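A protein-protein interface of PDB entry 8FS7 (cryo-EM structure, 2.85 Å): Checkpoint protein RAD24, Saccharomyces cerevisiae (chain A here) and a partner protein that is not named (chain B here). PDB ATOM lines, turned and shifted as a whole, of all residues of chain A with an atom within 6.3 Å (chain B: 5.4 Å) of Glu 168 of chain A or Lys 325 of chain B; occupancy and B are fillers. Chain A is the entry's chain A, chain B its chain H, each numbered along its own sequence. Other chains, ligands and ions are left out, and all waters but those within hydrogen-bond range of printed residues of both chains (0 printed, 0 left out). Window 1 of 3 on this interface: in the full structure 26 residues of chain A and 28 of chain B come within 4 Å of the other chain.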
ATOM      1  N   LEU A 160     -28.248 -15.506 -15.553  1.00  0.00           N
ATOM      2  CA  LEU A 160     -27.398 -14.329 -15.672  1.00  0.00           C
ATOM      3  C   LEU A 160     -27.373 -13.543 -14.369  1.00  0.00           C
ATOM      4  O   LEU A 160     -28.357 -12.875 -14.029  1.00  0.00           O
ATOM      5  CB  LEU A 160     -27.860 -13.427 -16.815  1.00  0.00           C
ATOM      6  CG  LEU A 160     -26.752 -12.692 -17.571  1.00  0.00           C
ATOM      7  CD1 LEU A 160     -25.843 -13.679 -18.276  1.00  0.00           C
ATOM      8  CD2 LEU A 160     -27.351 -11.711 -18.564  1.00  0.00           C
ATOM      9  N   GLU A 164     -23.024  -9.709 -14.295  1.00  0.00           N
ATOM     10  CA  GLU A 164     -22.561 -10.329 -15.529  1.00  0.00           C
ATOM     11  C   GLU A 164     -23.380  -9.921 -16.747  1.00  0.00           C
ATOM     12  O   GLU A 164     -23.026 -10.306 -17.867  1.00  0.00           O
ATOM     13  CB  GLU A 164     -22.585 -11.856 -15.394  1.00  0.00           C
ATOM     14  CG  GLU A 164     -21.547 -12.413 -14.433  1.00  0.00           C
ATOM     15  CD  GLU A 164     -20.167 -11.829 -14.662  1.00  0.00           C
ATOM     16  OE1 GLU A 164     -19.635 -11.978 -15.782  1.00  0.00           O
ATOM     17  OE2 GLU A 164     -19.615 -11.220 -13.721  1.00  0.00           O
ATOM     18  N   SER A 165     -24.460  -9.158 -16.555  1.00  0.00           N
ATOM     19  CA  SER A 165     -25.308  -8.768 -17.679  1.00  0.00           C
ATOM     20  C   SER A 165     -24.554  -7.876 -18.656  1.00  0.00           C
ATOM     21  O   SER A 165     -24.619  -8.077 -19.875  1.00  0.00           O
ATOM     22  CB  SER A 165     -26.565  -8.067 -17.165  1.00  0.00           C
ATOM     23  OG  SER A 165     -26.275  -6.748 -16.738  1.00  0.00           O
ATOM     24  N   PHE A 166     -23.820  -6.888 -18.139  1.00  0.00           N
ATOM     25  CA  PHE A 166     -23.065  -6.001 -19.016  1.00  0.00           C
ATOM     26  C   PHE A 166     -21.919  -6.738 -19.697  1.00  0.00           C
ATOM     27  O   PHE A 166     -21.600  -6.461 -20.859  1.00  0.00           O
ATOM     28  CB  PHE A 166     -22.533  -4.801 -18.234  1.00  0.00           C
ATOM     29  CG  PHE A 166     -21.830  -3.792 -19.093  1.00  0.00           C
ATOM     30  CD1 PHE A 166     -22.499  -3.163 -20.130  1.00  0.00           C
ATOM     31  CD2 PHE A 166     -20.497  -3.489 -18.880  1.00  0.00           C
ATOM     32  CE1 PHE A 166     -21.855  -2.238 -20.929  1.00  0.00           C
ATOM     33  CE2 PHE A 166     -19.847  -2.567 -19.678  1.00  0.00           C
ATOM     34  CZ  PHE A 166     -20.527  -1.939 -20.702  1.00  0.00           C
ATOM     35  N   SER A 167     -21.282  -7.673 -18.986  1.00  0.00           N
ATOM     36  CA  SER A 167     -20.227  -8.473 -19.598  1.00  0.00           C
ATOM     37  C   SER A 167     -20.770  -9.313 -20.746  1.00  0.00           C
ATOM     38  O   SER A 167     -20.162  -9.377 -21.821  1.00  0.00           O
ATOM     39  CB  SER A 167     -19.567  -9.366 -18.546  1.00  0.00           C
ATOM     40  OG  SER A 167     -18.493 -10.103 -19.104  1.00  0.00           O
ATOM     41  N   GLU A 168     -21.923  -9.956 -20.538  1.00  0.00           N
ATOM     42  CA  GLU A 168     -22.540 -10.734 -21.607  1.00  0.00           C
ATOM     43  C   GLU A 168     -22.941  -9.841 -22.775  1.00  0.00           C
ATOM     44  O   GLU A 168     -22.781 -10.224 -23.940  1.00  0.00           O
ATOM     45  CB  GLU A 168     -23.753 -11.495 -21.071  1.00  0.00           C
ATOM     46  CG  GLU A 168     -24.150 -12.698 -21.912  1.00  0.00           C
ATOM     47  CD  GLU A 168     -23.105 -13.795 -21.895  1.00  0.00           C
ATOM     48  OE1 GLU A 168     -22.416 -13.949 -20.865  1.00  0.00           O
ATOM     49  OE2 GLU A 168     -22.971 -14.506 -22.914  1.00  0.00           O
ATOM     50  N   PHE A 169     -23.460  -8.646 -22.480  1.00  0.00           N
ATOM     51  CA  PHE A 169     -23.820  -7.710 -23.541  1.00  0.00           C
ATOM     52  C   PHE A 169     -22.602  -7.311 -24.365  1.00  0.00           C
ATOM     53  O   PHE A 169     -22.662  -7.286 -25.598  1.00  0.00           O
ATOM     54  CB  PHE A 169     -24.488  -6.471 -22.944  1.00  0.00           C
ATOM     55  CG  PHE A 169     -24.462  -5.274 -23.852  1.00  0.00           C
ATOM     56  CD1 PHE A 169     -25.294  -5.210 -24.958  1.00  0.00           C
ATOM     57  CD2 PHE A 169     -23.605  -4.213 -23.602  1.00  0.00           C
ATOM     58  CE1 PHE A 169     -25.272  -4.112 -25.797  1.00  0.00           C
ATOM     59  CE2 PHE A 169     -23.579  -3.114 -24.439  1.00  0.00           C
ATOM     60  CZ  PHE A 169     -24.414  -3.064 -25.537  1.00  0.00           C
ATOM     61  N   LEU A 170     -21.487  -6.994 -23.699  1.00  0.00           N
ATOM     62  CA  LEU A 170     -20.276  -6.609 -24.418  1.00  0.00           C
ATOM     63  C   LEU A 170     -19.733  -7.764 -25.252  1.00  0.00           C
ATOM     64  O   LEU A 170     -19.318  -7.565 -26.402  1.00  0.00           O
ATOM     65  CB  LEU A 170     -19.213  -6.118 -23.437  1.00  0.00           C
ATOM     66  CG  LEU A 170     -19.259  -4.642 -23.038  1.00  0.00           C
ATOM     67  CD1 LEU A 170     -18.043  -4.287 -22.199  1.00  0.00           C
ATOM     68  CD2 LEU A 170     -19.347  -3.751 -24.266  1.00  0.00           C
ATOM     69  N   LYS A 171     -19.725  -8.975 -24.691  1.00  0.00           N
ATOM     70  CA  LYS A 171     -19.219 -10.128 -25.428  1.00  0.00           C
ATOM     71  C   LYS A 171     -20.087 -10.439 -26.641  1.00  0.00           C
ATOM     72  O   LYS A 171     -19.570 -10.795 -27.706  1.00  0.00           O
ATOM     73  CB  LYS A 171     -19.123 -11.338 -24.500  1.00  0.00           C
ATOM     74  CG  LYS A 171     -18.102 -11.166 -23.389  1.00  0.00           C
ATOM     75  CD  LYS A 171     -17.730 -12.493 -22.765  1.00  0.00           C
ATOM     76  CE  LYS A 171     -18.631 -12.813 -21.583  1.00  0.00           C
ATOM     77  NZ  LYS A 171     -18.121 -12.217 -20.317  1.00  0.00           N
ATOM     78  N   GLY A 172     -21.408 -10.314 -26.500  1.00  0.00           N
ATOM     79  CA  GLY A 172     -22.281 -10.507 -27.645  1.00  0.00           C
ATOM     80  C   GLY A 172     -22.134  -9.415 -28.688  1.00  0.00           C
ATOM     81  O   GLY A 172     -22.175  -9.686 -29.892  1.00  0.00           O
ATOM     82  N   ALA A 173     -21.959  -8.169 -28.244  1.00  0.00           N
ATOM     83  CA  ALA A 173     -21.864  -7.047 -29.169  1.00  0.00           C
ATOM     84  C   ALA A 173     -20.494  -6.945 -29.826  1.00  0.00           C
ATOM     85  O   ALA A 173     -20.344  -6.197 -30.797  1.00  0.00           O
ATOM     86  CB  ALA A 173     -22.193  -5.744 -28.441  1.00  0.00           C
ATOM     87  N   TYR A 175     -19.272  -9.139 -31.615  1.00  0.00           N
ATOM     88  CA  TYR A 175     -19.423  -9.823 -32.900  1.00  0.00           C
ATOM     89  C   TYR A 175     -20.222  -8.981 -33.891  1.00  0.00           C
ATOM     90  O   TYR A 175     -21.176  -9.455 -34.507  1.00  0.00           O
ATOM     91  CB  TYR A 175     -20.093 -11.176 -32.686  1.00  0.00           C
ATOM     92  CG  TYR A 175     -19.264 -12.175 -31.915  1.00  0.00           C
ATOM     93  CD1 TYR A 175     -19.335 -12.239 -30.530  1.00  0.00           C
ATOM     94  CD2 TYR A 175     -18.422 -13.062 -32.569  1.00  0.00           C
ATOM     95  CE1 TYR A 175     -18.585 -13.152 -29.818  1.00  0.00           C
ATOM     96  CE2 TYR A 175     -17.668 -13.981 -31.865  1.00  0.00           C
ATOM     97  CZ  TYR A 175     -17.755 -14.020 -30.490  1.00  0.00           C
ATOM     98  OH  TYR A 175     -17.007 -14.932 -29.785  1.00  0.00           O
ATOM     99  N   LEU A 204     -14.388  -3.735 -17.131  1.00  0.00           N
ATOM    100  CA  LEU A 204     -14.922  -4.281 -18.372  1.00  0.00           C
ATOM    101  C   LEU A 204     -14.691  -3.331 -19.539  1.00  0.00           C
ATOM    102  O   LEU A 204     -14.335  -3.772 -20.637  1.00  0.00           O
ATOM    103  CB  LEU A 204     -16.414  -4.573 -18.212  1.00  0.00           C
ATOM    104  CG  LEU A 204     -16.798  -5.999 -17.818  1.00  0.00           C
ATOM    105  CD1 LEU A 204     -18.287  -6.077 -17.534  1.00  0.00           C
ATOM    106  CD2 LEU A 204     -16.404  -6.984 -18.905  1.00  0.00           C
ATOM    107  N   ASP B 250     -15.699 -18.073 -22.002  1.00  0.00           N
ATOM    108  CA  ASP B 250     -16.797 -17.423 -22.704  1.00  0.00           C
ATOM    109  C   ASP B 250     -16.680 -17.526 -24.222  1.00  0.00           C
ATOM    110  O   ASP B 250     -17.200 -16.653 -24.931  1.00  0.00           O
ATOM    111  CB  ASP B 250     -16.888 -15.949 -22.290  1.00  0.00           C
ATOM    112  CG  ASP B 250     -15.566 -15.203 -22.450  1.00  0.00           C
ATOM    113  OD1 ASP B 250     -14.891 -15.360 -23.490  1.00  0.00           O
ATOM    114  OD2 ASP B 250     -15.207 -14.440 -21.532  1.00  0.00           O
ATOM    115  N   GLU B 251     -16.016 -18.553 -24.748  1.00  0.00           N
ATOM    116  CA  GLU B 251     -15.684 -18.571 -26.162  1.00  0.00           C
ATOM    117  C   GLU B 251     -15.491 -20.017 -26.604  1.00  0.00           C
ATOM    118  O   GLU B 251     -14.958 -20.845 -25.860  1.00  0.00           O
ATOM    119  CB  GLU B 251     -14.418 -17.742 -26.412  1.00  0.00           C
ATOM    120  CG  GLU B 251     -14.045 -17.501 -27.852  1.00  0.00           C
ATOM    121  CD  GLU B 251     -14.655 -16.208 -28.353  1.00  0.00           C
ATOM    122  OE1 GLU B 251     -14.475 -15.859 -29.534  1.00  0.00           O
ATOM    123  OE2 GLU B 251     -15.334 -15.535 -27.550  1.00  0.00           O
ATOM    124  N   VAL B 252     -15.923 -20.317 -27.827  1.00  0.00           N
ATOM    125  CA  VAL B 252     -15.836 -21.665 -28.384  1.00  0.00           C
ATOM    126  C   VAL B 252     -15.092 -21.608 -29.710  1.00  0.00           C
ATOM    127  O   VAL B 252     -15.462 -20.837 -30.603  1.00  0.00           O
ATOM    128  CB  VAL B 252     -17.225 -22.303 -28.574  1.00  0.00           C
ATOM    129  CG1 VAL B 252     -17.107 -23.609 -29.345  1.00  0.00           C
ATOM    130  CG2 VAL B 252     -17.866 -22.561 -27.229  1.00  0.00           C
ATOM    131  N   ILE B 323     -15.624 -19.737 -34.778  1.00  0.00           N
ATOM    132  CA  ILE B 323     -15.536 -19.269 -33.399  1.00  0.00           C
ATOM    133  C   ILE B 323     -16.841 -18.575 -33.031  1.00  0.00           C
ATOM    134  O   ILE B 323     -17.342 -17.744 -33.798  1.00  0.00           O
ATOM    135  CB  ILE B 323     -14.343 -18.315 -33.199  1.00  0.00           C
ATOM    136  CG1 ILE B 323     -13.038 -18.955 -33.670  1.00  0.00           C
ATOM    137  CG2 ILE B 323     -14.211 -17.938 -31.755  1.00  0.00           C
ATOM    138  CD1 ILE B 323     -11.825 -18.066 -33.504  1.00  0.00           C
ATOM    139  N   PHE B 324     -17.383 -18.903 -31.860  1.00  0.00           N
ATOM    140  CA  PHE B 324     -18.628 -18.301 -31.387  1.00  0.00           C
ATOM    141  C   PHE B 324     -18.689 -18.421 -29.866  1.00  0.00           C
ATOM    142  O   PHE B 324     -17.698 -18.762 -29.211  1.00  0.00           O
ATOM    143  CB  PHE B 324     -19.843 -18.944 -32.069  1.00  0.00           C
ATOM    144  CG  PHE B 324     -19.860 -20.446 -32.005  1.00  0.00           C
ATOM    145  CD1 PHE B 324     -19.206 -21.205 -32.963  1.00  0.00           C
ATOM    146  CD2 PHE B 324     -20.558 -21.099 -31.004  1.00  0.00           C
ATOM    147  CE1 PHE B 324     -19.229 -22.585 -32.907  1.00  0.00           C
ATOM    148  CE2 PHE B 324     -20.587 -22.478 -30.946  1.00  0.00           C
ATOM    149  CZ  PHE B 324     -19.922 -23.222 -31.898  1.00  0.00           C
ATOM    150  N   LYS B 325     -19.864 -18.137 -29.302  1.00  0.00           N
ATOM    151  CA  LYS B 325     -20.064 -18.085 -27.861  1.00  0.00           C
ATOM    152  C   LYS B 325     -20.211 -19.489 -27.275  1.00  0.00           C
ATOM    153  O   LYS B 325     -20.195 -20.498 -27.984  1.00  0.00           O
ATOM    154  CB  LYS B 325     -21.291 -17.240 -27.522  1.00  0.00           C
ATOM    155  CG  LYS B 325     -21.104 -15.752 -27.758  1.00  0.00           C
ATOM    156  CD  LYS B 325     -20.091 -15.164 -26.790  1.00  0.00           C
ATOM    157  CE  LYS B 325     -20.582 -15.243 -25.354  1.00  0.00           C
ATOM    158  NZ  LYS B 325     -21.892 -14.556 -25.170  1.00  0.00           N
ATOM    159  N   LEU B 326     -20.373 -19.542 -25.953  1.00  0.00           N
ATOM    160  CA  LEU B 326     -20.362 -20.795 -25.203  1.00  0.00           C
ATOM    161  C   LEU B 326     -21.668 -21.107 -24.489  1.00  0.00           C
ATOM    162  O   LEU B 326     -22.153 -22.237 -24.578  1.00  0.00           O
ATOM    163  CB  LEU B 326     -19.228 -20.774 -24.171  1.00  0.00           C
ATOM    164  CG  LEU B 326     -19.218 -21.900 -23.135  1.00  0.00           C
ATOM    165  CD1 LEU B 326     -18.569 -23.151 -23.699  1.00  0.00           C
ATOM    166  CD2 LEU B 326     -18.517 -21.462 -21.862  1.00  0.00           C
ATOM    167  N   LYS B 327     -22.245 -20.135 -23.775  1.00  0.00           N
ATOM    168  CA  LYS B 327     -23.403 -20.406 -22.923  1.00  0.00           C
ATOM    169  C   LYS B 327     -24.601 -20.877 -23.738  1.00  0.00           C
ATOM    170  O   LYS B 327     -25.291 -21.834 -23.359  1.00  0.00           O
ATOM    171  CB  LYS B 327     -23.766 -19.153 -22.129  1.00  0.00           C
ATOM    172  CG  LYS B 327     -24.916 -19.349 -21.159  1.00  0.00           C
ATOM    173  CD  LYS B 327     -25.266 -18.049 -20.462  1.00  0.00           C
ATOM    174  CE  LYS B 327     -25.636 -16.985 -21.482  1.00  0.00           C
ATOM    175  NZ  LYS B 327     -26.072 -15.717 -20.843  1.00  0.00           N
ATOM    176  N   ASP B 328     -24.870 -20.205 -24.860  1.00  0.00           N
ATOM    177  CA  ASP B 328     -26.003 -20.579 -25.699  1.00  0.00           C
ATOM    178  C   ASP B 328     -25.827 -21.984 -26.257  1.00  0.00           C
ATOM    179  O   ASP B 328     -26.791 -22.755 -26.338  1.00  0.00           O
ATOM    180  CB  ASP B 328     -26.174 -19.564 -26.828  1.00  0.00           C
ATOM    181  CG  ASP B 328     -26.301 -18.144 -26.316  1.00  0.00           C
ATOM    182  OD1 ASP B 328     -26.624 -17.968 -25.122  1.00  0.00           O
ATOM    183  OD2 ASP B 328     -26.070 -17.203 -27.103  1.00  0.00           O
ATOM    184  N   PHE B 329     -24.598 -22.334 -26.643  1.00  0.00           N
ATOM    185  CA  PHE B 329     -24.315 -23.689 -27.098  1.00  0.00           C
ATOM    186  C   PHE B 329     -24.565 -24.702 -25.986  1.00  0.00           C
ATOM    187  O   PHE B 329     -25.149 -25.766 -26.227  1.00  0.00           O
ATOM    188  CB  PHE B 329     -22.873 -23.776 -27.600  1.00  0.00           C
ATOM    189  CG  PHE B 329     -22.552 -25.055 -28.320  1.00  0.00           C
ATOM    190  CD1 PHE B 329     -23.527 -25.731 -29.036  1.00  0.00           C
ATOM    191  CD2 PHE B 329     -21.270 -25.578 -28.288  1.00  0.00           C
ATOM    192  CE1 PHE B 329     -23.229 -26.905 -29.700  1.00  0.00           C
ATOM    193  CE2 PHE B 329     -20.966 -26.751 -28.949  1.00  0.00           C
ATOM    194  CZ  PHE B 329     -21.947 -27.416 -29.657  1.00  0.00           C
ATOM    195  N   GLU B 375     -26.056 -18.706 -34.297  1.00  0.00           N
ATOM    196  CA  GLU B 375     -25.080 -17.903 -33.573  1.00  0.00           C
ATOM    197  C   GLU B 375     -24.194 -17.164 -34.561  1.00  0.00           C
ATOM    198  O   GLU B 375     -23.717 -17.751 -35.537  1.00  0.00           O
ATOM    199  CB  GLU B 375     -24.220 -18.766 -32.642  1.00  0.00           C
ATOM    200  CG  GLU B 375     -24.917 -19.187 -31.358  1.00  0.00           C
ATOM    201  CD  GLU B 375     -24.265 -18.598 -30.122  1.00  0.00           C
ATOM    202  OE1 GLU B 375     -24.333 -17.364 -29.940  1.00  0.00           O
ATOM    203  OE2 GLU B 375     -23.682 -19.370 -29.331  1.00  0.00           O
ATOM    204  N   VAL B 376     -23.970 -15.880 -34.300  1.00  0.00           N
ATOM    205  CA  VAL B 376     -23.104 -15.064 -35.144  1.00  0.00           C
ATOM    206  C   VAL B 376     -21.655 -15.411 -34.822  1.00  0.00           C
ATOM    207  O   VAL B 376     -21.232 -15.347 -33.663  1.00  0.00           O
ATOM    208  CB  VAL B 376     -23.378 -13.567 -34.936  1.00  0.00           C
ATOM    209  CG1 VAL B 376     -22.235 -12.732 -35.492  1.00  0.00           C
ATOM    210  CG2 VAL B 376     -24.696 -13.176 -35.586  1.00  0.00           C
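Among the printed residues, pairs that only touch across the chains: Leu 160 of chain A with Lys 327 of chain B (3.3 Å), Tyr 175 of chain A with Val 376 of chain B (3.6 Å), Tyr 175 of chain A with Phe 324 of chain B (3.9 Å) and Tyr 175 of chain A with Lys 325 of chain B (3.9 Å).
Printed residues of chain B that touch a printed residue of chain A: Asp 250, Glu 251, Phe 324, Lys 325, Lys 327 and Val 376. Hydrophobic or aromatic side chains of chain B within 4 Å of the printed part of chain A: Val 376. Of the 13 printed residues of chain A, 4 touch a printed residue of chain B. Among the printed residues, 8 pairs touch across the chains. Among the printed residues, Asp or Glu carboxylates within 4 Å of a Lys or Arg side-chain nitrogen of the other chain: Glu 168 of chain A with Lys 325 of chain B (2.5 Å), Glu 168 of chain A with Lys 327 of chain B (3.9 Å) and Lys 171 of chain A with Asp 250 of chain B (3.9 Å).
NZ of Lys 325 of chain B lies within salt-bridge range of OE2 of Glu 168 of chain A (2.5 Å). OH of Tyr 175 of chain A is in hydrogen-bond range of OE1 of Glu 251 of chain B. The side-chain amino group of Lys 171 of chain A lies within salt-bridge range of the side-chain carboxylate of Asp 250 of chain B (3.9 Å). The side-chain carboxylate (OE2) of Glu 168 of chain A lies within salt-bridge range of the side-chain amino group (NZ) of Lys 327 of chain B, 3.9 Å away.
The backbone NH (N) of Val 252 of chain B is in hydrogen-bond range of the backbone carbonyl oxygen (O) of Phe 324 of chain B, at 2.7 Å. OG of Ser 167 of chain A is in hydrogen-bond range of NZ of Lys 171 of chain A, 2.5 Å away.
Of chain B, only Lys 325 and Lys 327 come within 4 Å of Glu 168 of chain A. Printed residues of chain B within 4 Å of Lys 171 of chain A: Asp 250 (3.4 Å). Of the printed residues of chain B, Tyr 175 of chain A touches Glu 251 (2.7 Å), Phe 324 (3.9 Å), Lys 325 (3.9 Å) and Val 376 (3.6 Å). Lys 325 of chain B touches just these residues of chain A: Glu 168 and Tyr 175. Phe 329 of chain B touches none of the printed residues of chain A. The nearest residue of chain A that does not touch Lys 325 of chain B is Lys 171 of chain A (4.3 Å).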
